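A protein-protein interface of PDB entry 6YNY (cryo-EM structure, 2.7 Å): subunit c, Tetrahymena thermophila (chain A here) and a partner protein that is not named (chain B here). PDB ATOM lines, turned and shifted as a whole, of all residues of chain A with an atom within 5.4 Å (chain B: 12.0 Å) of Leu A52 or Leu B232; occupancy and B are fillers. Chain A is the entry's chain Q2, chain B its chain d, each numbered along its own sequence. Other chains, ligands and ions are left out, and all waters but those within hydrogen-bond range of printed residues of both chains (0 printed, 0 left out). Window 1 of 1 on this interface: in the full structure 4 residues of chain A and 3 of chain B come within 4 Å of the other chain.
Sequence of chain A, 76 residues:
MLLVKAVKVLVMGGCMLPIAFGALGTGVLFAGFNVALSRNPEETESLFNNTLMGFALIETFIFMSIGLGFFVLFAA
NH1 of Arg B234 is in hydrogen-bond range of O of Leu B232 (2.5 Å). The backbone carbonyl oxygen of Arg B234 is in hydrogen-bond range of the side-chain hydroxyl of Thr B228 (3.0 Å).
ND2 of Asn A49 touches CG of Arg B234, 3.1 Å away. Leu A52 touches Leu B232 (CD1 to CD1, 3.7 Å). CE of Met B231 touches CB of Ala A56, at 3.3 Å.
Of chain A, only Leu A52 (3.7 Å) comes within 4 Å of Leu B232. No residue of chain B comes within 4 Å of Asn A50. No residue of chain B comes within 4 Å of Phe A55. Of the printed residues of chain B, Asn A49 touches Arg B234. Of the printed residues of chain A, Arg B234 touches Asn A49. Phe A30 touches none of the printed residues of chain B. Asn B230 touches none of the printed residues of chain A. The nearest residue of chain B that does not touch Leu A52 is Arg B234 (4.2 Å). The nearest printed residue of chain A that does not touch Leu B232 is Phe A55 (6.2 Å). The nearest printed residue of chain A that does not touch Arg B234 is Leu A52 (4.2 Å).
Hydrophobic or aromatic side chains of chain A within 4 Å of the printed part of chain B: Leu A52 and Ala A56. Of the 12 printed residues of chain B, 3 touch a printed residue of chain A. Printed residues of chain B that touch a printed residue of chain A: Met B231, Leu B232 and Arg B234. Among the printed residues, 3 pairs touch across the chains. Among the printed residues, no Asp or Glu carboxylate lies within 4 Å of a Lys or Arg side-chain nitrogen of the other chain.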
ATOM      1  N   PHE A  30     -32.630 -12.694 -18.378  1.00  0.00           N
ATOM      2  CA  PHE A  30     -31.453 -11.840 -18.411  1.00  0.00           C
ATOM      3  C   PHE A  30     -31.719 -10.462 -17.826  1.00  0.00           C
ATOM      4  O   PHE A  30     -30.774  -9.800 -17.383  1.00  0.00           O
ATOM      5  CB  PHE A  30     -30.941 -11.716 -19.847  1.00  0.00           C
ATOM      6  CG  PHE A  30     -30.109 -12.884 -20.288  1.00  0.00           C
ATOM      7  CD1 PHE A  30     -28.734 -12.870 -20.126  1.00  0.00           C
ATOM      8  CD2 PHE A  30     -30.700 -14.002 -20.848  1.00  0.00           C
ATOM      9  CE1 PHE A  30     -27.965 -13.942 -20.523  1.00  0.00           C
ATOM     10  CE2 PHE A  30     -29.934 -15.080 -21.248  1.00  0.00           C
ATOM     11  CZ  PHE A  30     -28.564 -15.050 -21.083  1.00  0.00           C
ATOM     12  N   PHE A  48     -24.471 -16.347 -12.877  1.00  0.00           N
ATOM     13  CA  PHE A  48     -24.284 -16.596 -14.303  1.00  0.00           C
ATOM     14  C   PHE A  48     -24.509 -18.065 -14.639  1.00  0.00           C
ATOM     15  O   PHE A  48     -25.138 -18.389 -15.653  1.00  0.00           O
ATOM     16  CB  PHE A  48     -22.887 -16.155 -14.728  1.00  0.00           C
ATOM     17  CG  PHE A  48     -22.686 -16.135 -16.214  1.00  0.00           C
ATOM     18  CD1 PHE A  48     -22.801 -14.953 -16.924  1.00  0.00           C
ATOM     19  CD2 PHE A  48     -22.391 -17.298 -16.901  1.00  0.00           C
ATOM     20  CE1 PHE A  48     -22.619 -14.930 -18.288  1.00  0.00           C
ATOM     21  CE2 PHE A  48     -22.208 -17.281 -18.265  1.00  0.00           C
ATOM     22  CZ  PHE A  48     -22.324 -16.096 -18.961  1.00  0.00           C
ATOM     23  N   ASN A  49     -23.989 -18.968 -13.806  1.00  0.00           N
ATOM     24  CA  ASN A  49     -24.214 -20.393 -14.025  1.00  0.00           C
ATOM     25  C   ASN A  49     -25.703 -20.702 -14.082  1.00  0.00           C
ATOM     26  O   ASN A  49     -26.176 -21.386 -14.997  1.00  0.00           O
ATOM     27  CB  ASN A  49     -23.546 -21.208 -12.918  1.00  0.00           C
ATOM     28  CG  ASN A  49     -22.037 -21.065 -12.916  1.00  0.00           C
ATOM     29  OD1 ASN A  49     -21.429 -20.789 -11.882  1.00  0.00           O
ATOM     30  ND2 ASN A  49     -21.426 -21.251 -14.077  1.00  0.00           N
ATOM     31  N   ASN A  50     -26.461 -20.205 -13.103  1.00  0.00           N
ATOM     32  CA  ASN A  50     -27.892 -20.481 -13.062  1.00  0.00           C
ATOM     33  C   ASN A  50     -28.605 -19.909 -14.280  1.00  0.00           C
ATOM     34  O   ASN A  50     -29.635 -20.445 -14.704  1.00  0.00           O
ATOM     35  CB  ASN A  50     -28.491 -19.913 -11.777  1.00  0.00           C
ATOM     36  CG  ASN A  50     -27.759 -20.386 -10.541  1.00  0.00           C
ATOM     37  OD1 ASN A  50     -27.364 -19.584  -9.694  1.00  0.00           O
ATOM     38  ND2 ASN A  50     -27.568 -21.696 -10.430  1.00  0.00           N
ATOM     39  N   THR A  51     -28.079 -18.825 -14.851  1.00  0.00           N
ATOM     40  CA  THR A  51     -28.707 -18.219 -16.020  1.00  0.00           C
ATOM     41  C   THR A  51     -28.719 -19.191 -17.194  1.00  0.00           C
ATOM     42  O   THR A  51     -29.781 -19.546 -17.717  1.00  0.00           O
ATOM     43  CB  THR A  51     -27.974 -16.931 -16.394  1.00  0.00           C
ATOM     44  OG1 THR A  51     -28.099 -15.980 -15.329  1.00  0.00           O
ATOM     45  CG2 THR A  51     -28.537 -16.338 -17.677  1.00  0.00           C
ATOM     46  N   LEU A  52     -27.536 -19.632 -17.625  1.00  0.00           N
ATOM     47  CA  LEU A  52     -27.455 -20.521 -18.779  1.00  0.00           C
ATOM     48  C   LEU A  52     -28.191 -21.829 -18.525  1.00  0.00           C
ATOM     49  O   LEU A  52     -28.879 -22.343 -19.416  1.00  0.00           O
ATOM     50  CB  LEU A  52     -25.994 -20.778 -19.135  1.00  0.00           C
ATOM     51  CG  LEU A  52     -25.233 -19.532 -19.589  1.00  0.00           C
ATOM     52  CD1 LEU A  52     -23.778 -19.854 -19.866  1.00  0.00           C
ATOM     53  CD2 LEU A  52     -25.886 -18.922 -20.814  1.00  0.00           C
ATOM     54  N   MET A  53     -28.053 -22.396 -17.324  1.00  0.00           N
ATOM     55  CA  MET A  53     -28.783 -23.618 -17.006  1.00  0.00           C
ATOM     56  C   MET A  53     -30.278 -23.413 -17.213  1.00  0.00           C
ATOM     57  O   MET A  53     -30.940 -24.206 -17.893  1.00  0.00           O
ATOM     58  CB  MET A  53     -28.493 -24.054 -15.570  1.00  0.00           C
ATOM     59  CG  MET A  53     -28.900 -25.491 -15.282  1.00  0.00           C
ATOM     60  SD  MET A  53     -28.780 -25.951 -13.547  1.00  0.00           S
ATOM     61  CE  MET A  53     -30.242 -25.156 -12.895  1.00  0.00           C
ATOM     62  N   GLY A  54     -30.828 -22.347 -16.630  1.00  0.00           N
ATOM     63  CA  GLY A  54     -32.219 -22.013 -16.882  1.00  0.00           C
ATOM     64  C   GLY A  54     -32.496 -21.806 -18.359  1.00  0.00           C
ATOM     65  O   GLY A  54     -33.515 -22.264 -18.881  1.00  0.00           O
ATOM     66  N   PHE A  55     -31.589 -21.112 -19.051  1.00  0.00           N
ATOM     67  CA  PHE A  55     -31.738 -20.919 -20.489  1.00  0.00           C
ATOM     68  C   PHE A  55     -31.824 -22.254 -21.218  1.00  0.00           C
ATOM     69  O   PHE A  55     -32.605 -22.404 -22.165  1.00  0.00           O
ATOM     70  CB  PHE A  55     -30.568 -20.098 -21.028  1.00  0.00           C
ATOM     71  CG  PHE A  55     -30.599 -19.908 -22.514  1.00  0.00           C
ATOM     72  CD1 PHE A  55     -30.003 -20.831 -23.354  1.00  0.00           C
ATOM     73  CD2 PHE A  55     -31.220 -18.807 -23.070  1.00  0.00           C
ATOM     74  CE1 PHE A  55     -30.031 -20.659 -24.718  1.00  0.00           C
ATOM     75  CE2 PHE A  55     -31.253 -18.633 -24.437  1.00  0.00           C
ATOM     76  CZ  PHE A  55     -30.655 -19.559 -25.262  1.00  0.00           C
ATOM     77  N   ALA A  56     -31.020 -23.229 -20.798  1.00  0.00           N
ATOM     78  CA  ALA A  56     -31.044 -24.540 -21.436  1.00  0.00           C
ATOM     79  C   ALA A  56     -32.441 -25.138 -21.397  1.00  0.00           C
ATOM     80  O   ALA A  56     -32.988 -25.540 -22.430  1.00  0.00           O
ATOM     81  CB  ALA A  56     -30.053 -25.472 -20.747  1.00  0.00           C
ATOM     82  N   LEU A  57     -33.034 -25.208 -20.206  1.00  0.00           N
ATOM     83  CA  LEU A  57     -34.375 -25.765 -20.086  1.00  0.00           C
ATOM     84  C   LEU A  57     -35.363 -24.991 -20.947  1.00  0.00           C
ATOM     85  O   LEU A  57     -36.277 -25.577 -21.539  1.00  0.00           O
ATOM     86  CB  LEU A  57     -34.810 -25.746 -18.624  1.00  0.00           C
ATOM     87  CG  LEU A  57     -33.892 -26.506 -17.667  1.00  0.00           C
ATOM     88  CD1 LEU A  57     -34.318 -26.270 -16.230  1.00  0.00           C
ATOM     89  CD2 LEU A  57     -33.874 -27.984 -17.999  1.00  0.00           C
ATOM     90  N   LYS B 223      -5.968 -22.770 -25.196  1.00  0.00           N
ATOM     91  CA  LYS B 223      -7.380 -23.021 -24.950  1.00  0.00           C
ATOM     92  C   LYS B 223      -7.592 -24.421 -24.397  1.00  0.00           C
ATOM     93  O   LYS B 223      -6.972 -25.388 -24.846  1.00  0.00           O
ATOM     94  CB  LYS B 223      -8.189 -22.846 -26.233  1.00  0.00           C
ATOM     95  CG  LYS B 223      -8.621 -21.430 -26.510  1.00  0.00           C
ATOM     96  CD  LYS B 223      -9.689 -20.985 -25.535  1.00  0.00           C
ATOM     97  CE  LYS B 223     -10.166 -19.590 -25.848  1.00  0.00           C
ATOM     98  NZ  LYS B 223     -10.832 -19.524 -27.169  1.00  0.00           N
ATOM     99  N   CYS B 224      -8.478 -24.519 -23.419  1.00  0.00           N
ATOM    100  CA  CYS B 224      -8.860 -25.776 -22.802  1.00  0.00           C
ATOM    101  C   CYS B 224     -10.336 -26.037 -23.079  1.00  0.00           C
ATOM    102  O   CYS B 224     -11.025 -25.238 -23.715  1.00  0.00           O
ATOM    103  CB  CYS B 224      -8.576 -25.751 -21.299  1.00  0.00           C
ATOM    104  SG  CYS B 224      -6.899 -25.268 -20.861  1.00  0.00           S
ATOM    105  N   ALA B 225     -10.821 -27.172 -22.588  1.00  0.00           N
ATOM    106  CA  ALA B 225     -12.217 -27.539 -22.756  1.00  0.00           C
ATOM    107  C   ALA B 225     -12.542 -28.667 -21.796  1.00  0.00           C
ATOM    108  O   ALA B 225     -11.752 -29.600 -21.644  1.00  0.00           O
ATOM    109  CB  ALA B 225     -12.507 -27.966 -24.195  1.00  0.00           C
ATOM    110  N   LYS B 226     -13.704 -28.576 -21.154  1.00  0.00           N
ATOM    111  CA  LYS B 226     -14.122 -29.578 -20.191  1.00  0.00           C
ATOM    112  C   LYS B 226     -15.605 -29.864 -20.359  1.00  0.00           C
ATOM    113  O   LYS B 226     -16.356 -29.071 -20.930  1.00  0.00           O
ATOM    114  CB  LYS B 226     -13.835 -29.136 -18.754  1.00  0.00           C
ATOM    115  CG  LYS B 226     -14.629 -27.943 -18.299  1.00  0.00           C
ATOM    116  CD  LYS B 226     -14.292 -27.584 -16.872  1.00  0.00           C
ATOM    117  CE  LYS B 226     -15.071 -26.386 -16.408  1.00  0.00           C
ATOM    118  NZ  LYS B 226     -14.750 -26.050 -15.008  1.00  0.00           N
ATOM    119  N   ALA B 227     -16.009 -31.024 -19.854  1.00  0.00           N
ATOM    120  CA  ALA B 227     -17.398 -31.450 -19.840  1.00  0.00           C
ATOM    121  C   ALA B 227     -17.827 -31.683 -18.402  1.00  0.00           C
ATOM    122  O   ALA B 227     -17.135 -32.375 -17.649  1.00  0.00           O
ATOM    123  CB  ALA B 227     -17.593 -32.720 -20.658  1.00  0.00           C
ATOM    124  N   THR B 228     -18.957 -31.104 -18.025  1.00  0.00           N
ATOM    125  CA  THR B 228     -19.488 -31.210 -16.678  1.00  0.00           C
ATOM    126  C   THR B 228     -20.886 -31.811 -16.718  1.00  0.00           C
ATOM    127  O   THR B 228     -21.409 -32.166 -17.777  1.00  0.00           O
ATOM    128  CB  THR B 228     -19.516 -29.842 -15.996  1.00  0.00           C
ATOM    129  OG1 THR B 228     -20.404 -28.972 -16.704  1.00  0.00           O
ATOM    130  CG2 THR B 228     -18.140 -29.231 -15.976  1.00  0.00           C
ATOM    131  N   LYS B 229     -21.491 -31.926 -15.536  1.00  0.00           N
ATOM    132  CA  LYS B 229     -22.875 -32.371 -15.455  1.00  0.00           C
ATOM    133  C   LYS B 229     -23.821 -31.353 -16.070  1.00  0.00           C
ATOM    134  O   LYS B 229     -24.884 -31.722 -16.579  1.00  0.00           O
ATOM    135  CB  LYS B 229     -23.256 -32.627 -14.000  1.00  0.00           C
ATOM    136  CG  LYS B 229     -23.194 -31.399 -13.126  1.00  0.00           C
ATOM    137  CD  LYS B 229     -23.529 -31.729 -11.697  1.00  0.00           C
ATOM    138  CE  LYS B 229     -23.640 -30.485 -10.846  1.00  0.00           C
ATOM    139  NZ  LYS B 229     -24.784 -29.633 -11.258  1.00  0.00           N
ATOM    140  N   ASN B 230     -23.454 -30.080 -16.031  1.00  0.00           N
ATOM    141  CA  ASN B 230     -24.229 -29.021 -16.650  1.00  0.00           C
ATOM    142  C   ASN B 230     -23.731 -28.757 -18.065  1.00  0.00           C
ATOM    143  O   ASN B 230     -22.663 -29.215 -18.475  1.00  0.00           O
ATOM    144  CB  ASN B 230     -24.144 -27.753 -15.808  1.00  0.00           C
ATOM    145  CG  ASN B 230     -24.548 -27.984 -14.371  1.00  0.00           C
ATOM    146  OD1 ASN B 230     -25.507 -28.700 -14.089  1.00  0.00           O
ATOM    147  ND2 ASN B 230     -23.808 -27.386 -13.451  1.00  0.00           N
ATOM    148  N   MET B 231     -24.522 -28.004 -18.819  1.00  0.00           N
ATOM    149  CA  MET B 231     -24.168 -27.716 -20.197  1.00  0.00           C
ATOM    150  C   MET B 231     -23.163 -26.575 -20.271  1.00  0.00           C
ATOM    151  O   MET B 231     -22.980 -25.804 -19.326  1.00  0.00           O
ATOM    152  CB  MET B 231     -25.408 -27.364 -21.017  1.00  0.00           C
ATOM    153  CG  MET B 231     -26.175 -26.160 -20.525  1.00  0.00           C
ATOM    154  SD  MET B 231     -26.824 -25.179 -21.890  1.00  0.00           S
ATOM    155  CE  MET B 231     -27.671 -26.438 -22.836  1.00  0.00           C
ATOM    156  N   LEU B 232     -22.504 -26.477 -21.424  1.00  0.00           N
ATOM    157  CA  LEU B 232     -21.549 -25.408 -21.694  1.00  0.00           C
ATOM    158  C   LEU B 232     -20.383 -25.433 -20.715  1.00  0.00           C
ATOM    159  O   LEU B 232     -19.751 -24.407 -20.458  1.00  0.00           O
ATOM    160  CB  LEU B 232     -22.239 -24.045 -21.668  1.00  0.00           C
ATOM    161  CG  LEU B 232     -23.506 -23.967 -22.518  1.00  0.00           C
ATOM    162  CD1 LEU B 232     -24.202 -22.638 -22.333  1.00  0.00           C
ATOM    163  CD2 LEU B 232     -23.183 -24.197 -23.972  1.00  0.00           C
ATOM    164  N   GLY B 233     -20.085 -26.606 -20.163  1.00  0.00           N
ATOM    165  CA  GLY B 233     -18.971 -26.731 -19.250  1.00  0.00           C
ATOM    166  C   GLY B 233     -19.145 -26.008 -17.939  1.00  0.00           C
ATOM    167  O   GLY B 233     -18.161 -25.776 -17.235  1.00  0.00           O
ATOM    168  N   ARG B 234     -20.372 -25.645 -17.586  1.00  0.00           N
ATOM    169  CA  ARG B 234     -20.636 -24.968 -16.327  1.00  0.00           C
ATOM    170  C   ARG B 234     -21.053 -25.963 -15.252  1.00  0.00           C
ATOM    171  O   ARG B 234     -20.223 -26.695 -14.712  1.00  0.00           O
ATOM    172  CB  ARG B 234     -21.719 -23.907 -16.507  1.00  0.00           C
ATOM    173  CG  ARG B 234     -21.193 -22.547 -16.924  1.00  0.00           C
ATOM    174  CD  ARG B 234     -20.586 -22.573 -18.300  1.00  0.00           C
ATOM    175  NE  ARG B 234     -20.022 -21.281 -18.666  1.00  0.00           N
ATOM    176  CZ  ARG B 234     -19.468 -21.016 -19.842  1.00  0.00           C
ATOM    177  NH1 ARG B 234     -19.403 -21.952 -20.773  1.00  0.00           N
ATOM    178  NH2 ARG B 234     -18.979 -19.814 -20.087  1.00  0.00           N
